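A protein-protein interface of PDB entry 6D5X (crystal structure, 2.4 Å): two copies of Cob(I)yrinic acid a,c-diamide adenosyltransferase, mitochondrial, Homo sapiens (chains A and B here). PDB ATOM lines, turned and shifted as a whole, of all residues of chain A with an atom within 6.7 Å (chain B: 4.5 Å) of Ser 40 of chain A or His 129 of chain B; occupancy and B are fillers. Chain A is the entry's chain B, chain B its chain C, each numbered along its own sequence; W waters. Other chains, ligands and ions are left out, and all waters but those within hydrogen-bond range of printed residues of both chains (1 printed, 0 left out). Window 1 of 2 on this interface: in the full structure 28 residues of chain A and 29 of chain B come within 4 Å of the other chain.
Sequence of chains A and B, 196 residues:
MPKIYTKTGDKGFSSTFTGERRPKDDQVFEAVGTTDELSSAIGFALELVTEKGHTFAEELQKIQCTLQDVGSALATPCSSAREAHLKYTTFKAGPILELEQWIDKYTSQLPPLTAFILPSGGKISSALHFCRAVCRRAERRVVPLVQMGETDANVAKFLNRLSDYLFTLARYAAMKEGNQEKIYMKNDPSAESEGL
NH1 of Arg 132 of chain B is in salt-bridge range of OD1 of Asp 36 of chain A, 3.7 Å away.
The backbone carbonyl oxygen (O) of Pro 119 of chain B is in hydrogen-bond range of the side-chain amide nitrogen (NE2) of Gln 64 of chain A, at 3.4 Å.
N of Gly 43 of chain A sits close to NE2 of Gln 64 of chain A, 3.4 Å away.
The side-chain amide nitrogen (NE2) of Gln 64 of chain A sits at hydrogen-bond distance from the backbone carbonyl oxygen (O) of Ser 39 of chain A.
O of Asp 36 of chain A sits at hydrogen-bond distance from OG of Ser 40 of chain A.
CB of Ala 133 of chain B touches CA of Glu 37 of chain A (3.7 Å).
Ser 39 of chain A touches Pro 119 of chain B (OG to CD, 3.7 Å).
OG of Ser 40 of chain A touches CG of Pro 119 of chain B, 3.8 Å away.
O of His 129 of chain B touches OG of Ser 40 of chain A (3.5 Å).
CB of Ser 40 of chain A touches CA of Phe 130 of chain B (3.7 Å).
Pro 119 of chain B touches Gly 43 of chain A.
Gly 43 of chain A touches Ser 126 of chain B.
Phe 44 of chain A touches Ser 126 of chain B (CA to CB, 3.8 Å).
Printed residues of chain B within 4 Å of Glu 37 of chain A: Ala 133 (3.7 Å).
Ser 40 of chain A touches three residues of chain B.
Of the printed residues of chain B, Gln 64 of chain A touches Pro 119 (3.4 Å).
Ser 125 of chain B touches none of the printed residues of chain A.
His 129 of chain B touches just one residue of chain A: Ser 40 (3.5 Å).
Of the printed residues of chain A, Arg 132 of chain B touches Asp 36.
Ala 170 of chain B touches none of the printed residues of chain A.
The nearest printed residue of chain A that does not touch Pro 119 of chain B is Asp 36 of chain A (5.1 Å).
Of the 14 printed residues of chain A, 7 touch a printed residue of chain B.
Among the printed residues, Asp or Glu carboxylates within 4 Å of a Lys or Arg side-chain nitrogen of the other chain: Asp 36 of chain A with Arg 132 of chain B.
1 position is printed for both chains.
Water W1 lies within hydrogen-bond range of O of His 129 of chain B (2.9 Å) and OG of Ser 40 of chain A (3.3 Å).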
ATOM      1  N   THR A  35      23.959  16.029  23.433  1.00  0.00           N
ATOM      2  CA  THR A  35      22.944  16.924  23.982  1.00  0.00           C
ATOM      3  C   THR A  35      21.549  16.507  23.526  1.00  0.00           C
ATOM      4  O   THR A  35      20.586  16.518  24.312  1.00  0.00           O
ATOM      5  CB  THR A  35      23.236  18.361  23.552  1.00  0.00           C
ATOM      6  OG1 THR A  35      24.505  18.769  24.080  1.00  0.00           O
ATOM      7  CG2 THR A  35      22.152  19.302  24.056  1.00  0.00           C
ATOM      8  N   ASP A  36      21.432  16.112  22.256  1.00  0.00           N
ATOM      9  CA  ASP A  36      20.152  15.646  21.733  1.00  0.00           C
ATOM     10  C   ASP A  36      19.687  14.391  22.474  1.00  0.00           C
ATOM     11  O   ASP A  36      18.501  14.250  22.809  1.00  0.00           O
ATOM     12  CB  ASP A  36      20.301  15.376  20.234  1.00  0.00           C
ATOM     13  CG  ASP A  36      19.055  15.722  19.447  1.00  0.00           C
ATOM     14  OD1 ASP A  36      18.898  15.213  18.317  1.00  0.00           O
ATOM     15  OD2 ASP A  36      18.223  16.493  19.974  1.00  0.00           O
ATOM     16  N   GLU A  37      20.619  13.467  22.727  1.00  0.00           N
ATOM     17  CA  GLU A  37      20.307  12.238  23.453  1.00  0.00           C
ATOM     18  C   GLU A  37      19.824  12.537  24.868  1.00  0.00           C
ATOM     19  O   GLU A  37      18.889  11.894  25.365  1.00  0.00           O
ATOM     20  CB  GLU A  37      21.544  11.343  23.481  1.00  0.00           C
ATOM     21  CG  GLU A  37      21.298   9.910  23.897  1.00  0.00           C
ATOM     22  CD  GLU A  37      22.500   9.028  23.620  1.00  0.00           C
ATOM     23  OE1 GLU A  37      23.382   9.448  22.836  1.00  0.00           O
ATOM     24  OE2 GLU A  37      22.576   7.919  24.192  1.00  0.00           O
ATOM     25  N   LEU A  38      20.463  13.501  25.536  1.00  0.00           N
ATOM     26  CA  LEU A  38      20.008  13.913  26.863  1.00  0.00           C
ATOM     27  C   LEU A  38      18.580  14.441  26.806  1.00  0.00           C
ATOM     28  O   LEU A  38      17.739  14.100  27.653  1.00  0.00           O
ATOM     29  CB  LEU A  38      20.949  14.972  27.437  1.00  0.00           C
ATOM     30  CG  LEU A  38      20.469  15.676  28.711  1.00  0.00           C
ATOM     31  CD1 LEU A  38      20.215  14.674  29.839  1.00  0.00           C
ATOM     32  CD2 LEU A  38      21.470  16.723  29.149  1.00  0.00           C
ATOM     33  N   SER A  39      18.289  15.289  25.815  1.00  0.00           N
ATOM     34  CA  SER A  39      16.939  15.832  25.702  1.00  0.00           C
ATOM     35  C   SER A  39      15.914  14.721  25.485  1.00  0.00           C
ATOM     36  O   SER A  39      14.804  14.767  26.036  1.00  0.00           O
ATOM     37  CB  SER A  39      16.877  16.854  24.569  1.00  0.00           C
ATOM     38  OG  SER A  39      15.643  17.550  24.592  1.00  0.00           O
ATOM     39  N   SER A  40      16.285  13.689  24.721  1.00  0.00           N
ATOM     40  CA  SER A  40      15.352  12.590  24.469  1.00  0.00           C
ATOM     41  C   SER A  40      15.125  11.748  25.722  1.00  0.00           C
ATOM     42  O   SER A  40      14.000  11.290  25.985  1.00  0.00           O
ATOM     43  CB  SER A  40      15.875  11.714  23.334  1.00  0.00           C
ATOM     44  OG  SER A  40      15.964  12.457  22.134  1.00  0.00           O
ATOM     45  N   ALA A  41      16.188  11.512  26.494  1.00  0.00           N
ATOM     46  CA  ALA A  41      16.028  10.794  27.752  1.00  0.00           C
ATOM     47  C   ALA A  41      15.108  11.559  28.697  1.00  0.00           C
ATOM     48  O   ALA A  41      14.254  10.961  29.369  1.00  0.00           O
ATOM     49  CB  ALA A  41      17.393  10.552  28.395  1.00  0.00           C
ATOM     50  N   ILE A  42      15.254  12.884  28.743  1.00  0.00           N
ATOM     51  CA  ILE A  42      14.373  13.695  29.578  1.00  0.00           C
ATOM     52  C   ILE A  42      12.928  13.604  29.095  1.00  0.00           C
ATOM     53  O   ILE A  42      11.994  13.556  29.904  1.00  0.00           O
ATOM     54  CB  ILE A  42      14.874  15.151  29.621  1.00  0.00           C
ATOM     55  CG1 ILE A  42      16.133  15.249  30.483  1.00  0.00           C
ATOM     56  CG2 ILE A  42      13.796  16.084  30.139  1.00  0.00           C
ATOM     57  CD1 ILE A  42      16.751  16.625  30.485  1.00  0.00           C
ATOM     58  N   GLY A  43      12.718  13.569  27.776  1.00  0.00           N
ATOM     59  CA  GLY A  43      11.360  13.418  27.264  1.00  0.00           C
ATOM     60  C   GLY A  43      10.707  12.116  27.700  1.00  0.00           C
ATOM     61  O   GLY A  43       9.551  12.092  28.160  1.00  0.00           O
ATOM     62  N   PHE A  44      11.448  11.008  27.583  1.00  0.00           N
ATOM     63  CA  PHE A  44      10.870   9.738  28.012  1.00  0.00           C
ATOM     64  C   PHE A  44      10.592   9.748  29.511  1.00  0.00           C
ATOM     65  O   PHE A  44       9.543   9.264  29.955  1.00  0.00           O
ATOM     66  CB  PHE A  44      11.764   8.552  27.650  1.00  0.00           C
ATOM     67  CG  PHE A  44      11.155   7.225  28.022  1.00  0.00           C
ATOM     68  CD1 PHE A  44      11.525   6.567  29.185  1.00  0.00           C
ATOM     69  CD2 PHE A  44      10.162   6.667  27.231  1.00  0.00           C
ATOM     70  CE1 PHE A  44      10.936   5.359  29.534  1.00  0.00           C
ATOM     71  CE2 PHE A  44       9.574   5.461  27.571  1.00  0.00           C
ATOM     72  CZ  PHE A  44       9.959   4.807  28.724  1.00  0.00           C
ATOM     73  N   ALA A  45      11.527  10.279  30.308  1.00  0.00           N
ATOM     74  CA  ALA A  45      11.283  10.409  31.745  1.00  0.00           C
ATOM     75  C   ALA A  45      10.019  11.218  32.025  1.00  0.00           C
ATOM     76  O   ALA A  45       9.232  10.867  32.912  1.00  0.00           O
ATOM     77  CB  ALA A  45      12.492  11.045  32.430  1.00  0.00           C
ATOM     78  N   GLN A  64      14.535  21.253  28.343  1.00  0.00           N
ATOM     79  CA  GLN A  64      14.640  20.745  26.975  1.00  0.00           C
ATOM     80  C   GLN A  64      14.815  21.882  25.971  1.00  0.00           C
ATOM     81  O   GLN A  64      15.636  21.791  25.042  1.00  0.00           O
ATOM     82  CB  GLN A  64      13.413  19.905  26.622  1.00  0.00           C
ATOM     83  CG  GLN A  64      13.370  18.559  27.311  1.00  0.00           C
ATOM     84  CD  GLN A  64      12.206  17.711  26.835  1.00  0.00           C
ATOM     85  OE1 GLN A  64      11.047  18.059  27.055  1.00  0.00           O
ATOM     86  NE2 GLN A  64      12.510  16.592  26.186  1.00  0.00           N
ATOM     87  N   LEU A  67      18.240  23.029  26.129  1.00  0.00           N
ATOM     88  CA  LEU A  67      19.145  22.083  25.480  1.00  0.00           C
ATOM     89  C   LEU A  67      19.151  22.267  23.970  1.00  0.00           C
ATOM     90  O   LEU A  67      20.187  22.067  23.326  1.00  0.00           O
ATOM     91  CB  LEU A  67      18.771  20.644  25.843  1.00  0.00           C
ATOM     92  CG  LEU A  67      19.061  20.251  27.298  1.00  0.00           C
ATOM     93  CD1 LEU A  67      18.684  18.802  27.559  1.00  0.00           C
ATOM     94  CD2 LEU A  67      20.516  20.489  27.662  1.00  0.00           C
ATOM     95  N   CYS A 131      19.019   9.840  33.163  1.00  0.00           N
ATOM     96  CA  CYS A 131      19.209  11.152  32.547  1.00  0.00           C
ATOM     97  C   CYS A 131      20.461  11.838  33.076  1.00  0.00           C
ATOM     98  O   CYS A 131      21.180  12.504  32.323  1.00  0.00           O
ATOM     99  CB  CYS A 131      17.987  12.031  32.795  1.00  0.00           C
ATOM    100  SG  CYS A 131      16.489  11.454  32.002  1.00  0.00           S
ATOM    101  N   ILE B 117      10.431  20.542  17.051  1.00  0.00           N
ATOM    102  CA  ILE B 117       9.712  19.642  17.942  1.00  0.00           C
ATOM    103  C   ILE B 117      10.643  19.218  19.069  1.00  0.00           C
ATOM    104  O   ILE B 117      11.802  18.862  18.826  1.00  0.00           O
ATOM    105  CB  ILE B 117       9.175  18.423  17.173  1.00  0.00           C
ATOM    106  CG1 ILE B 117       7.955  18.817  16.345  1.00  0.00           C
ATOM    107  CG2 ILE B 117       8.808  17.299  18.111  1.00  0.00           C
ATOM    108  CD1 ILE B 117       7.483  17.714  15.446  1.00  0.00           C
ATOM    109  N   PRO B 119      11.444  16.371  22.014  1.00  0.00           N
ATOM    110  CA  PRO B 119      11.132  14.952  22.251  1.00  0.00           C
ATOM    111  C   PRO B 119       9.959  14.814  23.211  1.00  0.00           C
ATOM    112  O   PRO B 119      10.031  15.223  24.373  1.00  0.00           O
ATOM    113  CB  PRO B 119      12.431  14.402  22.851  1.00  0.00           C
ATOM    114  CG  PRO B 119      13.507  15.338  22.345  1.00  0.00           C
ATOM    115  CD  PRO B 119      12.856  16.690  22.295  1.00  0.00           C
ATOM    116  N   SER B 120       8.866  14.235  22.711  1.00  0.00           N
ATOM    117  CA  SER B 120       7.604  14.192  23.440  1.00  0.00           C
ATOM    118  C   SER B 120       6.568  13.392  22.661  1.00  0.00           C
ATOM    119  O   SER B 120       6.912  12.702  21.696  1.00  0.00           O
ATOM    120  CB  SER B 120       7.077  15.609  23.690  1.00  0.00           C
ATOM    121  OG  SER B 120       7.048  16.360  22.485  1.00  0.00           O
ATOM    122  N   SER B 125       6.214   7.630  21.193  1.00  0.00           N
ATOM    123  CA  SER B 125       6.882   8.712  20.481  1.00  0.00           C
ATOM    124  C   SER B 125       8.199   9.089  21.155  1.00  0.00           C
ATOM    125  O   SER B 125       9.226   9.257  20.486  1.00  0.00           O
ATOM    126  CB  SER B 125       5.942   9.914  20.385  1.00  0.00           C
ATOM    127  OG  SER B 125       6.541  10.994  19.694  1.00  0.00           O
ATOM    128  N   SER B 126       8.188   9.227  22.483  1.00  0.00           N
ATOM    129  CA  SER B 126       9.413   9.560  23.206  1.00  0.00           C
ATOM    130  C   SER B 126      10.462   8.462  23.066  1.00  0.00           C
ATOM    131  O   SER B 126      11.655   8.746  22.873  1.00  0.00           O
ATOM    132  CB  SER B 126       9.090   9.813  24.675  1.00  0.00           C
ATOM    133  OG  SER B 126       8.087  10.804  24.789  1.00  0.00           O
ATOM    134  N   ALA B 127      10.038   7.199  23.182  1.00  0.00           N
ATOM    135  CA  ALA B 127      10.963   6.089  22.987  1.00  0.00           C
ATOM    136  C   ALA B 127      11.586   6.133  21.596  1.00  0.00           C
ATOM    137  O   ALA B 127      12.787   5.875  21.435  1.00  0.00           O
ATOM    138  CB  ALA B 127      10.240   4.762  23.218  1.00  0.00           C
ATOM    139  N   LEU B 128      10.790   6.475  20.578  1.00  0.00           N
ATOM    140  CA  LEU B 128      11.331   6.549  19.224  1.00  0.00           C
ATOM    141  C   LEU B 128      12.270   7.735  19.051  1.00  0.00           C
ATOM    142  O   LEU B 128      13.233   7.648  18.281  1.00  0.00           O
ATOM    143  CB  LEU B 128      10.199   6.610  18.200  1.00  0.00           C
ATOM    144  CG  LEU B 128       9.400   5.312  18.064  1.00  0.00           C
ATOM    145  CD1 LEU B 128       8.188   5.524  17.180  1.00  0.00           C
ATOM    146  CD2 LEU B 128      10.275   4.189  17.514  1.00  0.00           C
ATOM    147  N   HIS B 129      12.035   8.834  19.772  1.00  0.00           N
ATOM    148  CA  HIS B 129      12.979   9.947  19.716  1.00  0.00           C
ATOM    149  C   HIS B 129      14.323   9.549  20.325  1.00  0.00           C
ATOM    150  O   HIS B 129      15.395   9.894  19.794  1.00  0.00           O
ATOM    151  CB  HIS B 129      12.406  11.161  20.447  1.00  0.00           C
ATOM    152  CG  HIS B 129      11.386  11.918  19.656  1.00  0.00           C
ATOM    153  ND1 HIS B 129      11.716  12.700  18.568  1.00  0.00           N
ATOM    154  CD2 HIS B 129      10.046  12.026  19.804  1.00  0.00           C
ATOM    155  CE1 HIS B 129      10.619  13.245  18.074  1.00  0.00           C
ATOM    156  NE2 HIS B 129       9.592  12.853  18.806  1.00  0.00           N
ATOM    157  N   PHE B 130      14.279   8.799  21.431  1.00  0.00           N
ATOM    158  CA  PHE B 130      15.512   8.290  22.027  1.00  0.00           C
ATOM    159  C   PHE B 130      16.232   7.338  21.074  1.00  0.00           C
ATOM    160  O   PHE B 130      17.465   7.398  20.926  1.00  0.00           O
ATOM    161  CB  PHE B 130      15.206   7.593  23.355  1.00  0.00           C
ATOM    162  CG  PHE B 130      16.428   7.053  24.052  1.00  0.00           C
ATOM    163  CD1 PHE B 130      17.303   7.906  24.706  1.00  0.00           C
ATOM    164  CD2 PHE B 130      16.704   5.694  24.048  1.00  0.00           C
ATOM    165  CE1 PHE B 130      18.431   7.413  25.344  1.00  0.00           C
ATOM    166  CE2 PHE B 130      17.829   5.194  24.687  1.00  0.00           C
ATOM    167  CZ  PHE B 130      18.694   6.056  25.335  1.00  0.00           C
ATOM    168  N   CYS B 131      15.476   6.441  20.435  1.00  0.00           N
ATOM    169  CA  CYS B 131      16.047   5.568  19.409  1.00  0.00           C
ATOM    170  C   CYS B 131      16.706   6.369  18.295  1.00  0.00           C
ATOM    171  O   CYS B 131      17.757   5.977  17.781  1.00  0.00           O
ATOM    172  CB  CYS B 131      14.969   4.651  18.835  1.00  0.00           C
ATOM    173  SG  CYS B 131      14.353   3.433  20.001  1.00  0.00           S
ATOM    174  N   ARG B 132      16.082   7.480  17.889  1.00  0.00           N
ATOM    175  CA  ARG B 132      16.657   8.316  16.840  1.00  0.00           C
ATOM    176  C   ARG B 132      18.004   8.888  17.267  1.00  0.00           C
ATOM    177  O   ARG B 132      18.955   8.949  16.469  1.00  0.00           O
ATOM    178  CB  ARG B 132      15.674   9.433  16.480  1.00  0.00           C
ATOM    179  CG  ARG B 132      16.191  10.430  15.461  1.00  0.00           C
ATOM    180  CD  ARG B 132      15.238  11.611  15.333  1.00  0.00           C
ATOM    181  NE  ARG B 132      15.614  12.511  14.247  1.00  0.00           N
ATOM    182  CZ  ARG B 132      16.338  13.611  14.415  1.00  0.00           C
ATOM    183  NH1 ARG B 132      16.756  13.948  15.626  1.00  0.00           N
ATOM    184  NH2 ARG B 132      16.644  14.375  13.375  1.00  0.00           N
ATOM    185  N   ALA B 133      18.116   9.280  18.535  1.00  0.00           N
ATOM    186  CA  ALA B 133      19.389   9.837  18.991  1.00  0.00           C
ATOM    187  C   ALA B 133      20.469   8.758  19.028  1.00  0.00           C
ATOM    188  O   ALA B 133      21.634   9.002  18.650  1.00  0.00           O
ATOM    189  CB  ALA B 133      19.230  10.480  20.365  1.00  0.00           C
ATOM    190  N   PHE B 167      12.185   9.636  13.203  1.00  0.00           N
ATOM    191  CA  PHE B 167      11.528  10.914  13.485  1.00  0.00           C
ATOM    192  C   PHE B 167      10.080  10.911  12.987  1.00  0.00           C
ATOM    193  O   PHE B 167       9.140  11.262  13.727  1.00  0.00           O
ATOM    194  CB  PHE B 167      12.320  12.054  12.835  1.00  0.00           C
ATOM    195  CG  PHE B 167      11.816  13.427  13.182  1.00  0.00           C
ATOM    196  CD1 PHE B 167      12.090  13.986  14.419  1.00  0.00           C
ATOM    197  CD2 PHE B 167      11.066  14.156  12.273  1.00  0.00           C
ATOM    198  CE1 PHE B 167      11.631  15.250  14.744  1.00  0.00           C
ATOM    199  CE2 PHE B 167      10.599  15.422  12.595  1.00  0.00           C
ATOM    200  CZ  PHE B 167      10.881  15.967  13.832  1.00  0.00           C
ATOM    201  N   ALA B 170       7.827   8.596  15.049  1.00  0.00           N
ATOM    202  CA  ALA B 170       7.452   9.224  16.313  1.00  0.00           C
ATOM    203  C   ALA B 170       6.288  10.188  16.111  1.00  0.00           C
ATOM    204  O   ALA B 170       5.310  10.178  16.877  1.00  0.00           O
ATOM    205  CB  ALA B 170       8.658   9.938  16.929  1.00  0.00           C
HETATM  206  O   HOH W   1      15.961  12.598  18.860  1.00  0.00           O
